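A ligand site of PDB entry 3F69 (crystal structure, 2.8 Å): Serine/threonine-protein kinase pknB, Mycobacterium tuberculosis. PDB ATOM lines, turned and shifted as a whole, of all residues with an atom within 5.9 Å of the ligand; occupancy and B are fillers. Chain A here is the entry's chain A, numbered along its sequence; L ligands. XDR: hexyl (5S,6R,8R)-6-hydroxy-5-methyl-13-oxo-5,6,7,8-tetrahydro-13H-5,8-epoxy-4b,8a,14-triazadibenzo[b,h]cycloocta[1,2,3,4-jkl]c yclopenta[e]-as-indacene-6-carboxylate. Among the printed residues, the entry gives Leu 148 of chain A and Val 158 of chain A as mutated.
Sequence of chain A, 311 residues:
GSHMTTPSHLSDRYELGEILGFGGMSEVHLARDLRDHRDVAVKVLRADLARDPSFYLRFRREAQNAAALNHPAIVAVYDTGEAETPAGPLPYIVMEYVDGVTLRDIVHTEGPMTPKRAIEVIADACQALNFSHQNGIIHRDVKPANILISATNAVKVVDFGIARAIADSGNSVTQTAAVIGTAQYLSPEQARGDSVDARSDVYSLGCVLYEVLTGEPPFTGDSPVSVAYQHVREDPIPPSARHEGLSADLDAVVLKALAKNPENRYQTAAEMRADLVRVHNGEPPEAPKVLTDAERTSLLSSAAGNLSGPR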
ATOM      1  N   LEU A  20       3.700 -16.406 -14.449  1.00  0.00           N
ATOM      2  CA  LEU A  20       4.005 -17.769 -14.009  1.00  0.00           C
ATOM      3  C   LEU A  20       2.813 -18.468 -13.361  1.00  0.00           C
ATOM      4  O   LEU A  20       2.695 -19.678 -13.412  1.00  0.00           O
ATOM      5  CB  LEU A  20       5.196 -17.762 -13.057  1.00  0.00           C
ATOM      6  CG  LEU A  20       6.534 -17.435 -13.724  1.00  0.00           C
ATOM      7  CD1 LEU A  20       7.648 -17.369 -12.696  1.00  0.00           C
ATOM      8  CD2 LEU A  20       6.827 -18.456 -14.806  1.00  0.00           C
ATOM      9  N   GLY A  21       1.925 -17.695 -12.744  1.00  0.00           N
ATOM     10  CA  GLY A  21       0.781 -18.267 -12.054  1.00  0.00           C
ATOM     11  C   GLY A  21      -0.091 -17.206 -11.426  1.00  0.00           C
ATOM     12  O   GLY A  21       0.343 -16.081 -11.199  1.00  0.00           O
ATOM     13  N   PHE A  22      -1.354 -17.539 -11.161  1.00  0.00           N
ATOM     14  CA  PHE A  22      -2.252 -16.629 -10.475  1.00  0.00           C
ATOM     15  C   PHE A  22      -2.480 -17.108  -9.065  1.00  0.00           C
ATOM     16  O   PHE A  22      -2.475 -18.312  -8.823  1.00  0.00           O
ATOM     17  CB  PHE A  22      -3.573 -16.537 -11.220  1.00  0.00           C
ATOM     18  CG  PHE A  22      -3.455 -15.914 -12.568  1.00  0.00           C
ATOM     19  CD1 PHE A  22      -3.185 -16.691 -13.685  1.00  0.00           C
ATOM     20  CD2 PHE A  22      -3.595 -14.543 -12.727  1.00  0.00           C
ATOM     21  CE1 PHE A  22      -3.072 -16.107 -14.936  1.00  0.00           C
ATOM     22  CE2 PHE A  22      -3.487 -13.959 -13.969  1.00  0.00           C
ATOM     23  CZ  PHE A  22      -3.222 -14.736 -15.077  1.00  0.00           C
ATOM     24  N   GLY A  23      -2.623 -16.183  -8.135  1.00  0.00           N
ATOM     25  CA  GLY A  23      -2.901 -16.520  -6.733  1.00  0.00           C
ATOM     26  C   GLY A  23      -4.165 -15.798  -6.319  1.00  0.00           C
ATOM     27  O   GLY A  23      -4.895 -15.293  -7.183  1.00  0.00           O
ATOM     28  N   VAL A  28       2.063 -13.770 -10.153  1.00  0.00           N
ATOM     29  CA  VAL A  28       3.514 -13.849 -10.223  1.00  0.00           C
ATOM     30  C   VAL A  28       4.047 -13.805 -11.660  1.00  0.00           C
ATOM     31  O   VAL A  28       3.619 -14.584 -12.503  1.00  0.00           O
ATOM     32  CB  VAL A  28       3.998 -15.118  -9.536  1.00  0.00           C
ATOM     33  CG1 VAL A  28       5.526 -15.184  -9.564  1.00  0.00           C
ATOM     34  CG2 VAL A  28       3.452 -15.178  -8.106  1.00  0.00           C
ATOM     35  N   ALA A  41      11.467 -13.823 -10.123  1.00  0.00           N
ATOM     36  CA  ALA A  41      10.003 -13.897 -10.113  1.00  0.00           C
ATOM     37  C   ALA A  41       9.512 -12.747  -9.267  1.00  0.00           C
ATOM     38  O   ALA A  41      10.038 -12.492  -8.181  1.00  0.00           O
ATOM     39  CB  ALA A  41       9.540 -15.197  -9.535  1.00  0.00           C
ATOM     40  N   LYS A  43       6.090 -11.097  -7.543  1.00  0.00           N
ATOM     41  CA  LYS A  43       4.700 -11.264  -7.146  1.00  0.00           C
ATOM     42  C   LYS A  43       4.118  -9.870  -6.961  1.00  0.00           C
ATOM     43  O   LYS A  43       4.654  -9.086  -6.185  1.00  0.00           O
ATOM     44  CB  LYS A  43       4.635 -12.020  -5.833  1.00  0.00           C
ATOM     45  CG  LYS A  43       3.243 -12.249  -5.269  1.00  0.00           C
ATOM     46  CD  LYS A  43       3.374 -12.997  -3.941  1.00  0.00           C
ATOM     47  CE  LYS A  43       2.069 -13.648  -3.499  1.00  0.00           C
ATOM     48  NZ  LYS A  43       2.050 -13.847  -2.021  1.00  0.00           N
ATOM     49  N   VAL A  75      12.083 -21.468  -2.132  1.00  0.00           N
ATOM     50  CA  VAL A  75      12.290 -20.360  -3.058  1.00  0.00           C
ATOM     51  C   VAL A  75      12.627 -19.107  -2.254  1.00  0.00           C
ATOM     52  O   VAL A  75      11.848 -18.690  -1.413  1.00  0.00           O
ATOM     53  CB  VAL A  75      11.032 -20.118  -3.956  1.00  0.00           C
ATOM     54  CG1 VAL A  75      11.254 -18.954  -4.918  1.00  0.00           C
ATOM     55  CG2 VAL A  75      10.676 -21.372  -4.725  1.00  0.00           C
ATOM     56  N   MET A  95      11.408 -12.545  -5.990  1.00  0.00           N
ATOM     57  CA  MET A  95      11.845 -13.868  -5.501  1.00  0.00           C
ATOM     58  C   MET A  95      12.688 -14.666  -6.484  1.00  0.00           C
ATOM     59  O   MET A  95      12.725 -14.386  -7.687  1.00  0.00           O
ATOM     60  CB  MET A  95      10.635 -14.716  -5.153  1.00  0.00           C
ATOM     61  CG  MET A  95       9.667 -14.036  -4.265  1.00  0.00           C
ATOM     62  SD  MET A  95       8.218 -15.053  -3.962  1.00  0.00           S
ATOM     63  CE  MET A  95       8.951 -16.402  -3.033  1.00  0.00           C
ATOM     64  N   GLU A  96      13.368 -15.684  -5.953  1.00  0.00           N
ATOM     65  CA  GLU A  96      14.033 -16.688  -6.757  1.00  0.00           C
ATOM     66  C   GLU A  96      13.104 -17.222  -7.855  1.00  0.00           C
ATOM     67  O   GLU A  96      11.958 -17.552  -7.608  1.00  0.00           O
ATOM     68  CB  GLU A  96      14.473 -17.847  -5.861  1.00  0.00           C
ATOM     69  CG  GLU A  96      15.378 -18.872  -6.504  1.00  0.00           C
ATOM     70  CD  GLU A  96      15.607 -20.095  -5.588  1.00  0.00           C
ATOM     71  OE1 GLU A  96      15.470 -19.954  -4.351  1.00  0.00           O
ATOM     72  OE2 GLU A  96      15.908 -21.199  -6.125  1.00  0.00           O
ATOM     73  N   TYR A  97      13.624 -17.299  -9.078  1.00  0.00           N
ATOM     74  CA  TYR A  97      12.875 -17.837 -10.183  1.00  0.00           C
ATOM     75  C   TYR A  97      13.256 -19.308 -10.399  1.00  0.00           C
ATOM     76  O   TYR A  97      14.409 -19.703 -10.325  1.00  0.00           O
ATOM     77  CB  TYR A  97      13.114 -17.003 -11.434  1.00  0.00           C
ATOM     78  CG  TYR A  97      12.740 -17.677 -12.742  1.00  0.00           C
ATOM     79  CD1 TYR A  97      13.720 -18.030 -13.654  1.00  0.00           C
ATOM     80  CD2 TYR A  97      11.396 -17.940 -13.073  1.00  0.00           C
ATOM     81  CE1 TYR A  97      13.400 -18.642 -14.862  1.00  0.00           C
ATOM     82  CE2 TYR A  97      11.062 -18.549 -14.277  1.00  0.00           C
ATOM     83  CZ  TYR A  97      12.079 -18.905 -15.170  1.00  0.00           C
ATOM     84  OH  TYR A  97      11.803 -19.506 -16.388  1.00  0.00           O
ATOM     85  N   VAL A  98      12.234 -20.119 -10.619  1.00  0.00           N
ATOM     86  CA  VAL A  98      12.411 -21.539 -10.817  1.00  0.00           C
ATOM     87  C   VAL A  98      11.904 -21.856 -12.213  1.00  0.00           C
ATOM     88  O   VAL A  98      10.695 -21.784 -12.502  1.00  0.00           O
ATOM     89  CB  VAL A  98      11.628 -22.341  -9.751  1.00  0.00           C
ATOM     90  CG1 VAL A  98      11.701 -23.820 -10.042  1.00  0.00           C
ATOM     91  CG2 VAL A  98      12.166 -22.029  -8.373  1.00  0.00           C
ATOM     92  N   ASP A  99      12.840 -22.183 -13.090  1.00  0.00           N
ATOM     93  CA  ASP A  99      12.532 -22.590 -14.453  1.00  0.00           C
ATOM     94  C   ASP A  99      11.975 -23.991 -14.383  1.00  0.00           C
ATOM     95  O   ASP A  99      12.735 -24.959 -14.454  1.00  0.00           O
ATOM     96  CB  ASP A  99      13.844 -22.549 -15.248  1.00  0.00           C
ATOM     97  CG  ASP A  99      13.686 -23.036 -16.682  1.00  0.00           C
ATOM     98  OD1 ASP A  99      12.536 -23.245 -17.123  1.00  0.00           O
ATOM     99  OD2 ASP A  99      14.728 -23.194 -17.370  1.00  0.00           O
ATOM    100  N   GLY A 100      10.669 -24.135 -14.224  1.00  0.00           N
ATOM    101  CA  GLY A 100      10.094 -25.463 -14.070  1.00  0.00           C
ATOM    102  C   GLY A 100       8.585 -25.516 -14.162  1.00  0.00           C
ATOM    103  O   GLY A 100       7.987 -24.709 -14.863  1.00  0.00           O
ATOM    104  N   VAL A 101       7.962 -26.479 -13.473  1.00  0.00           N
ATOM    105  CA  VAL A 101       6.495 -26.636 -13.468  1.00  0.00           C
ATOM    106  C   VAL A 101       6.043 -27.087 -12.108  1.00  0.00           C
ATOM    107  O   VAL A 101       6.824 -27.591 -11.318  1.00  0.00           O
ATOM    108  CB  VAL A 101       6.010 -27.692 -14.489  1.00  0.00           C
ATOM    109  CG1 VAL A 101       6.369 -27.295 -15.935  1.00  0.00           C
ATOM    110  CG2 VAL A 101       6.590 -29.067 -14.153  1.00  0.00           C
ATOM    111  N   THR A 102       4.764 -26.906 -11.817  1.00  0.00           N
ATOM    112  CA  THR A 102       4.236 -27.294 -10.517  1.00  0.00           C
ATOM    113  C   THR A 102       3.965 -28.800 -10.459  1.00  0.00           C
ATOM    114  O   THR A 102       3.724 -29.448 -11.479  1.00  0.00           O
ATOM    115  CB  THR A 102       2.905 -26.560 -10.240  1.00  0.00           C
ATOM    116  OG1 THR A 102       1.921 -26.958 -11.202  1.00  0.00           O
ATOM    117  CG2 THR A 102       3.098 -25.067 -10.340  1.00  0.00           C
ATOM    118  N   ARG A 104       1.239 -29.793  -9.428  1.00  0.00           N
ATOM    119  CA  ARG A 104      -0.130 -29.871  -9.924  1.00  0.00           C
ATOM    120  C   ARG A 104      -0.131 -30.146 -11.422  1.00  0.00           C
ATOM    121  O   ARG A 104      -0.948 -30.931 -11.905  1.00  0.00           O
ATOM    122  CB  ARG A 104      -0.917 -28.604  -9.615  1.00  0.00           C
ATOM    123  CG  ARG A 104      -2.354 -28.678 -10.089  1.00  0.00           C
ATOM    124  CD  ARG A 104      -2.856 -27.304 -10.531  1.00  0.00           C
ATOM    125  NE  ARG A 104      -4.311 -27.239 -10.600  1.00  0.00           N
ATOM    126  CZ  ARG A 104      -5.038 -27.659 -11.642  1.00  0.00           C
ATOM    127  NH1 ARG A 104      -4.468 -28.198 -12.713  1.00  0.00           N
ATOM    128  NH2 ARG A 104      -6.368 -27.544 -11.597  1.00  0.00           N
ATOM    129  N   ASP A 105       0.779 -29.512 -12.167  1.00  0.00           N
ATOM    130  CA  ASP A 105       0.856 -29.723 -13.610  1.00  0.00           C
ATOM    131  C   ASP A 105       1.334 -31.120 -13.964  1.00  0.00           C
ATOM    132  O   ASP A 105       0.798 -31.764 -14.869  1.00  0.00           O
ATOM    133  CB  ASP A 105       1.770 -28.678 -14.254  1.00  0.00           C
ATOM    134  CG  ASP A 105       1.146 -27.280 -14.260  1.00  0.00           C
ATOM    135  OD1 ASP A 105      -0.093 -27.221 -14.544  1.00  0.00           O
ATOM    136  OD2 ASP A 105       1.885 -26.265 -13.990  1.00  0.00           O
ATOM    137  N   LYS A 143       0.601 -27.892  -0.914  1.00  0.00           N
ATOM    138  CA  LYS A 143      -0.335 -28.405  -1.891  1.00  0.00           C
ATOM    139  C   LYS A 143       0.373 -28.435  -3.238  1.00  0.00           C
ATOM    140  O   LYS A 143       1.365 -27.728  -3.425  1.00  0.00           O
ATOM    141  CB  LYS A 143      -1.577 -27.542  -1.923  1.00  0.00           C
ATOM    142  CG  LYS A 143      -1.345 -26.154  -2.472  1.00  0.00           C
ATOM    143  CD  LYS A 143      -2.521 -25.221  -2.125  1.00  0.00           C
ATOM    144  CE  LYS A 143      -2.716 -24.182  -3.236  1.00  0.00           C
ATOM    145  NZ  LYS A 143      -3.192 -22.847  -2.725  1.00  0.00           N
ATOM    146  N   ALA A 145       0.112 -27.245  -6.112  1.00  0.00           N
ATOM    147  CA  ALA A 145       0.393 -26.005  -6.835  1.00  0.00           C
ATOM    148  C   ALA A 145       1.452 -25.148  -6.129  1.00  0.00           C
ATOM    149  O   ALA A 145       1.858 -24.136  -6.660  1.00  0.00           O
ATOM    150  CB  ALA A 145      -0.865 -25.215  -7.072  1.00  0.00           C
ATOM    151  N   ASN A 146       1.897 -25.532  -4.946  1.00  0.00           N
ATOM    152  CA  ASN A 146       2.839 -24.697  -4.235  1.00  0.00           C
ATOM    153  C   ASN A 146       4.171 -25.399  -4.125  1.00  0.00           C
ATOM    154  O   ASN A 146       5.074 -24.937  -3.441  1.00  0.00           O
ATOM    155  CB  ASN A 146       2.314 -24.293  -2.841  1.00  0.00           C
ATOM    156  CG  ASN A 146       1.411 -23.057  -2.878  1.00  0.00           C
ATOM    157  OD1 ASN A 146       1.472 -22.275  -3.819  1.00  0.00           O
ATOM    158  ND2 ASN A 146       0.565 -22.897  -1.859  1.00  0.00           N
ATOM    159  N   LEU A 148       7.231 -26.710  -6.581  1.00  0.00           N
ATOM    160  CA  LEU A 148       7.757 -26.623  -7.952  1.00  0.00           C
ATOM    161  C   LEU A 148       8.814 -27.675  -8.220  1.00  0.00           C
ATOM    162  O   LEU A 148       9.643 -27.966  -7.350  1.00  0.00           O
ATOM    163  CB  LEU A 148       8.381 -25.251  -8.192  1.00  0.00           C
ATOM    164  CG  LEU A 148       7.541 -24.008  -7.958  1.00  0.00           C
ATOM    165  CD1 LEU A 148       8.379 -22.767  -8.248  1.00  0.00           C
ATOM    166  CD2 LEU A 148       6.316 -24.041  -8.839  1.00  0.00           C
ATOM    167  N   VAL A 158       7.109 -22.968  -2.651  1.00  0.00           N
ATOM    168  CA  VAL A 158       6.790 -21.540  -2.630  1.00  0.00           C
ATOM    169  C   VAL A 158       5.572 -21.230  -1.768  1.00  0.00           C
ATOM    170  O   VAL A 158       4.785 -22.123  -1.446  1.00  0.00           O
ATOM    171  CB  VAL A 158       6.446 -21.004  -4.036  1.00  0.00           C
ATOM    172  CG1 VAL A 158       7.553 -21.295  -5.013  1.00  0.00           C
ATOM    173  CG2 VAL A 158       5.125 -21.613  -4.519  1.00  0.00           C
ATOM    174  N   ASP A 159       5.396 -19.964  -1.429  1.00  0.00           N
ATOM    175  CA  ASP A 159       4.152 -19.500  -0.845  1.00  0.00           C
ATOM    176  C   ASP A 159       3.963 -19.834   0.638  1.00  0.00           C
ATOM    177  O   ASP A 159       2.876 -20.207   1.084  1.00  0.00           O
ATOM    178  CB  ASP A 159       2.973 -20.022  -1.656  1.00  0.00           C
ATOM    179  CG  ASP A 159       1.687 -19.294  -1.355  1.00  0.00           C
ATOM    180  OD1 ASP A 159       1.712 -18.131  -0.857  1.00  0.00           O
ATOM    181  OD2 ASP A 159       0.629 -19.892  -1.652  1.00  0.00           O
HETATM  182  CAR XDR L   1      -1.273 -21.939  -9.700  1.00  0.00           C
HETATM  183  OAV XDR L   1       0.132 -21.655  -9.290  1.00  0.00           O
HETATM  184  CAY XDR L   1       0.402 -21.287  -7.995  1.00  0.00           C
HETATM  185  OAD XDR L   1      -0.512 -21.154  -7.183  1.00  0.00           O
HETATM  186  CBM XDR L   1       1.843 -21.254  -7.532  1.00  0.00           C
HETATM  187  OAE XDR L   1       2.088 -20.964  -6.175  1.00  0.00           O
HETATM  188  CAT XDR L   1       2.957 -21.661  -8.511  1.00  0.00           C
HETATM  189  CBL XDR L   1       2.846 -20.822  -9.790  1.00  0.00           C
HETATM  190  OAW XDR L   1       2.151 -19.664  -9.369  1.00  0.00           O
HETATM  191  CBN XDR L   1       2.150 -19.745  -7.934  1.00  0.00           C
HETATM  192  CAB XDR L   1       1.094 -18.727  -7.485  1.00  0.00           C
HETATM  193  NBK XDR L   1       3.471 -19.155  -7.464  1.00  0.00           N
HETATM  194  CBE XDR L   1       3.604 -18.411  -6.349  1.00  0.00           C
HETATM  195  CAM XDR L   1       2.684 -18.020  -5.392  1.00  0.00           C
HETATM  196  CAI XDR L   1       3.103 -17.230  -4.316  1.00  0.00           C
HETATM  197  CAF XDR L   1       4.444 -16.853  -4.196  1.00  0.00           C
HETATM  198  CAJ XDR L   1       5.376 -17.247  -5.158  1.00  0.00           C
HETATM  199  CBB XDR L   1       4.942 -18.025  -6.219  1.00  0.00           C
HETATM  200  CBF XDR L   1       5.626 -18.552  -7.296  1.00  0.00           C
HETATM  201  CBI XDR L   1       4.667 -19.241  -8.032  1.00  0.00           C
HETATM  202  CBH XDR L   1       5.059 -19.886  -9.180  1.00  0.00           C
HETATM  203  NBJ XDR L   1       4.285 -20.577  -9.999  1.00  0.00           N
HETATM  204  CBD XDR L   1       5.058 -21.064 -10.970  1.00  0.00           C
HETATM  205  CAL XDR L   1       4.743 -21.866 -12.071  1.00  0.00           C
HETATM  206  CAH XDR L   1       5.750 -22.277 -12.937  1.00  0.00           C
HETATM  207  CAG XDR L   1       7.053 -21.852 -12.734  1.00  0.00           C
HETATM  208  CAK XDR L   1       7.372 -21.001 -11.674  1.00  0.00           C
HETATM  209  CBC XDR L   1       6.381 -20.632 -10.778  1.00  0.00           C
HETATM  210  CBG XDR L   1       6.385 -19.853  -9.617  1.00  0.00           C
HETATM  211  CBA XDR L   1       7.368 -19.178  -8.892  1.00  0.00           C
HETATM  212  CAZ XDR L   1       6.961 -18.521  -7.729  1.00  0.00           C
HETATM  213  CAS XDR L   1       8.145 -17.819  -7.100  1.00  0.00           C
HETATM  214  NAU XDR L   1       9.230 -18.179  -8.013  1.00  0.00           N
HETATM  215  CAX XDR L   1       8.756 -18.934  -9.026  1.00  0.00           C
HETATM  216  OAC XDR L   1       9.505 -19.376  -9.918  1.00  0.00           O
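OD1 of Asn 146 sits at hydrogen-bond distance from OAE of the ligand (2.8 Å). O of Ala 145 sits close to OAE of the ligand (3.2 Å). OAC of the ligand lies within hydrogen-bond range of N of Val 98, at 2.9 Å.
The side-chain carboxylate (OD2) of Asp 105 is in hydrogen-bond range of the side-chain hydroxyl (OG1) of Thr 102, 2.9 Å away. The backbone NH of Leu 20 lies within hydrogen-bond range of the backbone carbonyl oxygen of Val 28, at 2.7 Å. N of Val 158 is in hydrogen-bond range of O of Asn 146. The backbone NH (N) of Val 28 lies within hydrogen-bond range of the backbone carbonyl oxygen (O) of Gly 21. The side-chain amide nitrogen (ND2) of Asn 146 sits at hydrogen-bond distance from the side-chain carboxylate (OD2) of Asp 159 (3.0 Å). The backbone carbonyl oxygen (O) of Ala 41 sits at hydrogen-bond distance from the backbone NH (N) of Met 95, at 2.6 Å. The side-chain hydroxyl (OG1) of Thr 102 sits close to the backbone NH (N) of Arg 104 (3.4 Å).
A nitrogen (NAU) of the ligand sits close to the backbone carbonyl oxygen (O) of Glu 96 (2.8 Å). Leu 20 touches the ligand (O to CAL, 3.3 Å). CA of Gly 21 touches OAW of the ligand (3.3 Å). Phe 22 touches the ligand (O to OAD, 3.8 Å). CG2 of Val 28 touches CBE of the ligand, 3.7 Å away. Ala 41 touches the ligand (CB to NAU, 3.4 Å). CE of Lys 43 touches CAI of the ligand, at 3.8 Å. Val 75 touches the ligand (CG1 to NAU, 3.8 Å). Met 95 touches the ligand. Tyr 97 touches the ligand (CA to OAC, 3.7 Å). O of Gly 100 touches CAG of the ligand (3.7 Å). Thr 102 touches the ligand. Leu 148 touches the ligand. Val 158 touches the ligand. OD1 of Asp 159 touches CAI of the ligand, 3.8 Å away. Hydrophobic or aromatic side chains that line the ligand: Leu 20, Val 28, Ala 41, Val 75, Met 95, Tyr 97, Val 98, Leu 148 and Val 158. Of the 24 residues printed, 18 come within 4 Å of the ligand.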
